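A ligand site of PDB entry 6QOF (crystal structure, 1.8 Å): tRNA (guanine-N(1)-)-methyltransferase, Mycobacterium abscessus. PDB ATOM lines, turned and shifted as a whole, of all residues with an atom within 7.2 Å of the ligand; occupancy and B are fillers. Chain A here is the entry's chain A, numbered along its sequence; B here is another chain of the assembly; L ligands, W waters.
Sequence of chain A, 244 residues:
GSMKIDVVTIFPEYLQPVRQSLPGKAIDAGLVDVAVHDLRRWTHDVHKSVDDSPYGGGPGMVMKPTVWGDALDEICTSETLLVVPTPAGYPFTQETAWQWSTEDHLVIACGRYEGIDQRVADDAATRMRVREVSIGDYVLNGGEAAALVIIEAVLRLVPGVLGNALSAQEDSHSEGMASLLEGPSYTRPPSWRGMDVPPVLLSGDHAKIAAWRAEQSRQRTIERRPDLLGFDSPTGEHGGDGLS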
ATOM      1  N   VAL A  84      15.192  24.858   3.591  1.00  0.00           N
ATOM      2  CA  VAL A  84      16.283  23.933   3.294  1.00  0.00           C
ATOM      3  C   VAL A  84      16.299  23.656   1.796  1.00  0.00           C
ATOM      4  O   VAL A  84      15.498  22.886   1.318  1.00  0.00           O
ATOM      5  CB  VAL A  84      16.127  22.605   4.050  1.00  0.00           C
ATOM      6  CG1 VAL A  84      17.366  21.718   3.817  1.00  0.00           C
ATOM      7  CG2 VAL A  84      15.866  22.855   5.544  1.00  0.00           C
ATOM      8  N   PRO A  85      17.188  24.336   1.058  1.00  0.00           N
ATOM      9  CA  PRO A  85      17.206  24.071  -0.378  1.00  0.00           C
ATOM     10  C   PRO A  85      17.767  22.695  -0.638  1.00  0.00           C
ATOM     11  O   PRO A  85      18.820  22.321  -0.093  1.00  0.00           O
ATOM     12  CB  PRO A  85      18.127  25.165  -0.932  1.00  0.00           C
ATOM     13  CG  PRO A  85      18.191  26.218   0.158  1.00  0.00           C
ATOM     14  CD  PRO A  85      18.038  25.478   1.436  1.00  0.00           C
ATOM     15  N   THR A  86      17.043  21.930  -1.445  1.00  0.00           N
ATOM     16  CA  THR A  86      17.455  20.587  -1.796  1.00  0.00           C
ATOM     17  C   THR A  86      16.776  20.190  -3.097  1.00  0.00           C
ATOM     18  O   THR A  86      15.616  20.528  -3.305  1.00  0.00           O
ATOM     19  CB  THR A  86      17.132  19.555  -0.683  1.00  0.00           C
ATOM     20  OG1 THR A  86      17.196  18.246  -1.241  1.00  0.00           O
ATOM     21  CG2 THR A  86      15.723  19.767  -0.103  1.00  0.00           C
ATOM     22  N   PRO A  87      17.502  19.464  -3.971  1.00  0.00           N
ATOM     23  CA  PRO A  87      16.849  19.094  -5.233  1.00  0.00           C
ATOM     24  C   PRO A  87      15.740  18.067  -5.025  1.00  0.00           C
ATOM     25  O   PRO A  87      14.973  17.808  -5.946  1.00  0.00           O
ATOM     26  CB  PRO A  87      18.015  18.529  -6.067  1.00  0.00           C
ATOM     27  CG  PRO A  87      18.971  17.992  -5.052  1.00  0.00           C
ATOM     28  CD  PRO A  87      18.875  18.955  -3.878  1.00  0.00           C
ATOM     29  N   ALA A  88      15.664  17.495  -3.825  1.00  0.00           N
ATOM     30  CA  ALA A  88      14.580  16.584  -3.476  1.00  0.00           C
ATOM     31  C   ALA A  88      13.409  17.292  -2.791  1.00  0.00           C
ATOM     32  O   ALA A  88      12.519  16.639  -2.246  1.00  0.00           O
ATOM     33  CB  ALA A  88      15.124  15.458  -2.562  1.00  0.00           C
ATOM     34  N   GLY A  89      13.412  18.625  -2.816  1.00  0.00           N
ATOM     35  CA  GLY A  89      12.399  19.386  -2.107  1.00  0.00           C
ATOM     36  C   GLY A  89      11.110  19.573  -2.891  1.00  0.00           C
ATOM     37  O   GLY A  89      10.997  19.185  -4.060  1.00  0.00           O
ATOM     38  N   GLY A 111      23.235  23.262   2.329  1.00  0.00           N
ATOM     39  CA  GLY A 111      24.037  22.049   2.463  1.00  0.00           C
ATOM     40  C   GLY A 111      24.297  21.401   1.122  1.00  0.00           C
ATOM     41  O   GLY A 111      23.655  21.735   0.122  1.00  0.00           O
ATOM     42  N   ARG A 112      25.246  20.469   1.104  1.00  0.00           N
ATOM     43  CA  ARG A 112      25.573  19.740  -0.126  1.00  0.00           C
ATOM     44  C   ARG A 112      24.351  18.968  -0.609  1.00  0.00           C
ATOM     45  O   ARG A 112      23.499  18.566   0.186  1.00  0.00           O
ATOM     46  CB  ARG A 112      26.758  18.809   0.102  1.00  0.00           C
ATOM     47  CG  ARG A 112      26.563  17.820   1.241  1.00  0.00           C
ATOM     48  CD  ARG A 112      27.881  17.070   1.518  1.00  0.00           C
ATOM     49  NE  ARG A 112      28.337  16.370   0.307  1.00  0.00           N
ATOM     50  CZ  ARG A 112      29.613  16.124   0.008  1.00  0.00           C
ATOM     51  NH1 ARG A 112      30.573  16.518   0.822  1.00  0.00           N
ATOM     52  NH2 ARG A 112      29.913  15.478  -1.107  1.00  0.00           N
ATOM     53  N   TYR A 113      24.273  18.743  -1.915  1.00  0.00           N
ATOM     54  CA  TYR A 113      23.032  18.220  -2.477  1.00  0.00           C
ATOM     55  C   TYR A 113      22.684  16.807  -1.976  1.00  0.00           C
ATOM     56  O   TYR A 113      21.502  16.449  -1.948  1.00  0.00           O
ATOM     57  CB  TYR A 113      23.105  18.233  -4.005  1.00  0.00           C
ATOM     58  CG  TYR A 113      23.809  17.061  -4.610  1.00  0.00           C
ATOM     59  CD1 TYR A 113      25.191  17.073  -4.820  1.00  0.00           C
ATOM     60  CD2 TYR A 113      23.098  15.933  -4.992  1.00  0.00           C
ATOM     61  CE1 TYR A 113      25.830  15.994  -5.385  1.00  0.00           C
ATOM     62  CE2 TYR A 113      23.733  14.846  -5.554  1.00  0.00           C
ATOM     63  CZ  TYR A 113      25.085  14.886  -5.758  1.00  0.00           C
ATOM     64  OH  TYR A 113      25.708  13.796  -6.314  1.00  0.00           O
ATOM     65  N   GLU A 114      23.683  16.030  -1.586  1.00  0.00           N
ATOM     66  CA  GLU A 114      23.441  14.674  -1.085  1.00  0.00           C
ATOM     67  C   GLU A 114      22.592  14.723   0.183  1.00  0.00           C
ATOM     68  O   GLU A 114      21.898  13.757   0.507  1.00  0.00           O
ATOM     69  CB  GLU A 114      24.741  13.933  -0.803  1.00  0.00           C
ATOM     70  CG  GLU A 114      25.601  13.683  -2.033  1.00  0.00           C
ATOM     71  CD  GLU A 114      26.631  14.775  -2.234  1.00  0.00           C
ATOM     72  OE1 GLU A 114      26.414  15.910  -1.731  1.00  0.00           O
ATOM     73  OE2 GLU A 114      27.656  14.508  -2.877  1.00  0.00           O
ATOM     74  N   VAL A 133      12.871  22.759  -0.177  1.00  0.00           N
ATOM     75  CA  VAL A 133      12.448  23.211  -1.500  1.00  0.00           C
ATOM     76  C   VAL A 133      13.523  23.089  -2.569  1.00  0.00           C
ATOM     77  O   VAL A 133      14.701  23.321  -2.304  1.00  0.00           O
ATOM     78  CB  VAL A 133      11.976  24.686  -1.473  1.00  0.00           C
ATOM     79  CG1 VAL A 133      10.666  24.815  -0.662  1.00  0.00           C
ATOM     80  CG2 VAL A 133      13.079  25.617  -0.943  1.00  0.00           C
ATOM     81  N   SER A 134      13.076  22.738  -3.776  1.00  0.00           N
ATOM     82  CA  SER A 134      13.953  22.714  -4.951  1.00  0.00           C
ATOM     83  C   SER A 134      13.682  23.933  -5.808  1.00  0.00           C
ATOM     84  O   SER A 134      12.528  24.321  -5.974  1.00  0.00           O
ATOM     85  CB  SER A 134      13.724  21.430  -5.759  1.00  0.00           C
ATOM     86  OG  SER A 134      14.381  21.515  -7.011  1.00  0.00           O
ATOM     87  N   ILE A 135      14.729  24.537  -6.373  1.00  0.00           N
ATOM     88  CA  ILE A 135      14.489  25.691  -7.240  1.00  0.00           C
ATOM     89  C   ILE A 135      14.429  25.309  -8.707  1.00  0.00           C
ATOM     90  O   ILE A 135      14.198  26.169  -9.558  1.00  0.00           O
ATOM     91  CB  ILE A 135      15.562  26.796  -7.098  1.00  0.00           C
ATOM     92  CG1 ILE A 135      16.960  26.280  -7.454  1.00  0.00           C
ATOM     93  CG2 ILE A 135      15.512  27.422  -5.684  1.00  0.00           C
ATOM     94  CD1 ILE A 135      17.928  27.395  -7.845  1.00  0.00           C
ATOM     95  N   GLY A 136      14.604  24.022  -8.995  1.00  0.00           N
ATOM     96  CA  GLY A 136      14.493  23.572 -10.371  1.00  0.00           C
ATOM     97  C   GLY A 136      14.990  22.158 -10.565  1.00  0.00           C
ATOM     98  O   GLY A 136      15.585  21.547  -9.662  1.00  0.00           O
ATOM     99  N   ASP A 137      14.756  21.637 -11.766  1.00  0.00           N
ATOM    100  CA  ASP A 137      15.094  20.258 -12.090  1.00  0.00           C
ATOM    101  C   ASP A 137      16.528  20.097 -12.603  1.00  0.00           C
ATOM    102  O   ASP A 137      16.758  19.688 -13.741  1.00  0.00           O
ATOM    103  CB  ASP A 137      14.105  19.716 -13.124  1.00  0.00           C
ATOM    104  CG  ASP A 137      12.687  19.675 -12.596  1.00  0.00           C
ATOM    105  OD1 ASP A 137      12.504  19.243 -11.438  1.00  0.00           O
ATOM    106  OD2 ASP A 137      11.759  20.081 -13.319  1.00  0.00           O
ATOM    107  N   TYR A 138      17.484  20.427 -11.752  1.00  0.00           N
ATOM    108  CA  TYR A 138      18.889  20.281 -12.058  1.00  0.00           C
ATOM    109  C   TYR A 138      19.562  20.143 -10.717  1.00  0.00           C
ATOM    110  O   TYR A 138      18.969  20.471  -9.678  1.00  0.00           O
ATOM    111  CB  TYR A 138      19.444  21.485 -12.829  1.00  0.00           C
ATOM    112  CG  TYR A 138      18.824  22.778 -12.350  1.00  0.00           C
ATOM    113  CD1 TYR A 138      19.229  23.368 -11.156  1.00  0.00           C
ATOM    114  CD2 TYR A 138      17.817  23.404 -13.090  1.00  0.00           C
ATOM    115  CE1 TYR A 138      18.644  24.546 -10.689  1.00  0.00           C
ATOM    116  CE2 TYR A 138      17.233  24.588 -12.635  1.00  0.00           C
ATOM    117  CZ  TYR A 138      17.655  25.146 -11.441  1.00  0.00           C
ATOM    118  OH  TYR A 138      17.080  26.303 -10.985  1.00  0.00           O
ATOM    119  N   VAL A 139      20.795  19.647 -10.724  1.00  0.00           N
ATOM    120  CA  VAL A 139      21.517  19.472  -9.472  1.00  0.00           C
ATOM    121  C   VAL A 139      22.669  20.478  -9.395  1.00  0.00           C
ATOM    122  O   VAL A 139      23.475  20.601 -10.321  1.00  0.00           O
ATOM    123  CB  VAL A 139      22.055  18.032  -9.335  1.00  0.00           C
ATOM    124  CG1 VAL A 139      23.061  17.913  -8.165  1.00  0.00           C
ATOM    125  CG2 VAL A 139      20.903  17.073  -9.124  1.00  0.00           C
ATOM    126  N   LEU A 140      22.706  21.210  -8.281  1.00  0.00           N
ATOM    127  CA  LEU A 140      23.866  22.034  -7.917  1.00  0.00           C
ATOM    128  C   LEU A 140      24.664  21.261  -6.885  1.00  0.00           C
ATOM    129  O   LEU A 140      24.121  20.389  -6.213  1.00  0.00           O
ATOM    130  CB  LEU A 140      23.433  23.381  -7.350  1.00  0.00           C
ATOM    131  CG  LEU A 140      22.326  24.066  -8.149  1.00  0.00           C
ATOM    132  CD1 LEU A 140      21.898  25.365  -7.463  1.00  0.00           C
ATOM    133  CD2 LEU A 140      22.786  24.325  -9.579  1.00  0.00           C
ATOM    134  N   ASN A 141      25.951  21.571  -6.735  1.00  0.00           N
ATOM    135  CA  ASN A 141      26.753  20.848  -5.749  1.00  0.00           C
ATOM    136  C   ASN A 141      26.222  21.042  -4.333  1.00  0.00           C
ATOM    137  O   ASN A 141      26.359  20.166  -3.484  1.00  0.00           O
ATOM    138  CB  ASN A 141      28.213  21.271  -5.816  1.00  0.00           C
ATOM    139  CG  ASN A 141      29.112  20.142  -6.288  1.00  0.00           C
ATOM    140  OD1 ASN A 141      28.652  19.213  -6.958  1.00  0.00           O
ATOM    141  ND2 ASN A 141      30.379  20.189  -5.909  1.00  0.00           N
ATOM    142  N   GLY A 142      25.627  22.204  -4.089  1.00  0.00           N
ATOM    143  CA  GLY A 142      25.053  22.523  -2.792  1.00  0.00           C
ATOM    144  C   GLY A 142      23.976  23.588  -2.916  1.00  0.00           C
ATOM    145  O   GLY A 142      23.733  24.134  -4.002  1.00  0.00           O
ATOM    146  N   GLY A 143      23.328  23.883  -1.793  1.00  0.00           N
ATOM    147  CA  GLY A 143      22.196  24.799  -1.796  1.00  0.00           C
ATOM    148  C   GLY A 143      22.538  26.274  -1.889  1.00  0.00           C
ATOM    149  O   GLY A 143      21.618  27.105  -1.938  1.00  0.00           O
ATOM    150  N   GLU A 144      23.832  26.601  -1.923  1.00  0.00           N
ATOM    151  CA  GLU A 144      24.286  27.994  -1.912  1.00  0.00           C
ATOM    152  C   GLU A 144      23.656  28.876  -3.002  1.00  0.00           C
ATOM    153  O   GLU A 144      23.049  29.912  -2.705  1.00  0.00           O
ATOM    154  CB  GLU A 144      25.806  28.058  -2.035  1.00  0.00           C
ATOM    155  CG  GLU A 144      26.529  27.861  -0.690  1.00  0.00           C
ATOM    156  CD  GLU A 144      26.455  26.426  -0.186  1.00  0.00           C
ATOM    157  OE1 GLU A 144      26.268  25.512  -1.024  1.00  0.00           O
ATOM    158  OE2 GLU A 144      26.596  26.209   1.036  1.00  0.00           O
ATOM    159  N   ALA A 145      23.813  28.484  -4.269  1.00  0.00           N
ATOM    160  CA  ALA A 145      23.238  29.279  -5.363  1.00  0.00           C
ATOM    161  C   ALA A 145      21.711  29.290  -5.296  1.00  0.00           C
ATOM    162  O   ALA A 145      21.100  30.282  -5.692  1.00  0.00           O
ATOM    163  CB  ALA A 145      23.722  28.739  -6.729  1.00  0.00           C
ATOM    164  N   ALA A 146      21.111  28.205  -4.809  1.00  0.00           N
ATOM    165  CA  ALA A 146      19.658  28.145  -4.625  1.00  0.00           C
ATOM    166  C   ALA A 146      19.214  29.148  -3.584  1.00  0.00           C
ATOM    167  O   ALA A 146      18.155  29.757  -3.704  1.00  0.00           O
ATOM    168  CB  ALA A 146      19.228  26.736  -4.213  1.00  0.00           C
ATOM    169  N   ALA A 147      20.019  29.311  -2.536  1.00  0.00           N
ATOM    170  CA  ALA A 147      19.723  30.343  -1.539  1.00  0.00           C
ATOM    171  C   ALA A 147      19.749  31.747  -2.149  1.00  0.00           C
ATOM    172  O   ALA A 147      18.900  32.581  -1.820  1.00  0.00           O
ATOM    173  CB  ALA A 147      20.692  30.263  -0.374  1.00  0.00           C
ATOM    174  N   ILE A 150      16.512  32.187  -4.036  1.00  0.00           N
ATOM    175  CA  ILE A 150      15.362  32.329  -3.149  1.00  0.00           C
ATOM    176  C   ILE A 150      15.347  33.747  -2.558  1.00  0.00           C
ATOM    177  O   ILE A 150      14.319  34.419  -2.573  1.00  0.00           O
ATOM    178  CB  ILE A 150      15.395  31.256  -2.040  1.00  0.00           C
ATOM    179  CG1 ILE A 150      15.061  29.903  -2.648  1.00  0.00           C
ATOM    180  CG2 ILE A 150      14.423  31.610  -0.920  1.00  0.00           C
ATOM    181  CD1 ILE A 150      15.412  28.705  -1.761  1.00  0.00           C
ATOM    182  N   VAL B 149      23.389  30.108 -11.048  1.00  0.00           N
ATOM    183  CA  VAL B 149      22.832  28.763 -10.973  1.00  0.00           C
ATOM    184  C   VAL B 149      23.274  27.955 -12.177  1.00  0.00           C
ATOM    185  O   VAL B 149      23.663  26.794 -12.051  1.00  0.00           O
ATOM    186  CB  VAL B 149      21.294  28.797 -10.863  1.00  0.00           C
ATOM    187  CG1 VAL B 149      20.665  27.471 -11.258  1.00  0.00           C
ATOM    188  CG2 VAL B 149      20.885  29.160  -9.412  1.00  0.00           C
HETATM  189  N1  LIG L   1      20.877  22.011  -4.060  1.00  0.00           N
HETATM  190  C1  LIG L   1      21.392  21.364  -5.131  1.00  0.00           C
HETATM  191  N2  LIG L   1      20.524  21.429  -6.157  1.00  0.00           N
HETATM  192  C2  LIG L   1      19.404  22.124  -5.733  1.00  0.00           C
HETATM  193  C3  LIG L   1      18.178  22.517  -6.344  1.00  0.00           C
HETATM  194  N3  LIG L   1      17.850  22.187  -7.680  1.00  0.00           N
HETATM  195  N4  LIG L   1      17.291  23.202  -5.616  1.00  0.00           N
HETATM  196  C4  LIG L   1      17.535  23.538  -4.335  1.00  0.00           C
HETATM  197  N5  LIG L   1      18.679  23.207  -3.725  1.00  0.00           N
HETATM  198  C5  LIG L   1      19.634  22.481  -4.418  1.00  0.00           C
HETATM  199  O   HOH W   1      21.351  21.372  -1.430  1.00  0.00           O
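N of Val 133 is in hydrogen-bond range of O of Val 84, 3.0 Å away. The backbone NH of Tyr 113 lies within hydrogen-bond range of the backbone carbonyl oxygen of Asn 141. The backbone NH (N) of Gly 143 lies within hydrogen-bond range of the backbone carbonyl oxygen (O) of Gly 111. The backbone carbonyl oxygen (O) of Gly 136 is in hydrogen-bond range of the side-chain hydroxyl (OG) of Ser 134 (2.9 Å). OH of Tyr 138 is in hydrogen-bond range of O of Ile 135 (3.2 Å). OG1 of Thr 86 sits close to N of Ala 88 (3.1 Å). The backbone NH (N) of Ser 134 lies close to the backbone carbonyl oxygen (O) of Thr 86 (3.4 Å). The backbone NH (N) of Thr 86 sits at hydrogen-bond distance from the backbone carbonyl oxygen (O) of Val 133 (2.9 Å).
Merely in contact with the ligand: Pro 85 (3.3 Å), Ser 134 (3.4 Å), Val 133 (3.5 Å), Gly 142 (3.6 Å), Ala 146 (3.6 Å), Pro 87 (3.6 Å), Tyr 113 (3.7 Å), Gly 143 (3.8 Å) and Val 139 (3.98 Å). Of the 27 residues printed, 14 come within 4 Å of the ligand. The nearest printed residue that does not touch the ligand is Asn 141 (4.8 Å).
The backbone carbonyl oxygen (O) of Tyr 138 sits at hydrogen-bond distance from a nitrogen (N3) of the ligand (2.9 Å). A nitrogen (N5) of the ligand is in hydrogen-bond range of the backbone NH of Thr 86. A nitrogen (N4) of the ligand sits at hydrogen-bond distance from the backbone NH of Ile 135. The backbone NH (N) of Leu 140 is in hydrogen-bond range of a nitrogen (N2) of the ligand (3.1 Å). The backbone carbonyl oxygen (O) of Gly 136 lies within hydrogen-bond range of a nitrogen (N3) of the ligand.
Water W1 lies within hydrogen-bond range of N1 of the ligand (2.7 Å), O of Gly 111 (2.8 Å), O of Pro 85 (3.0 Å) and N of Gly 143 (3.2 Å).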
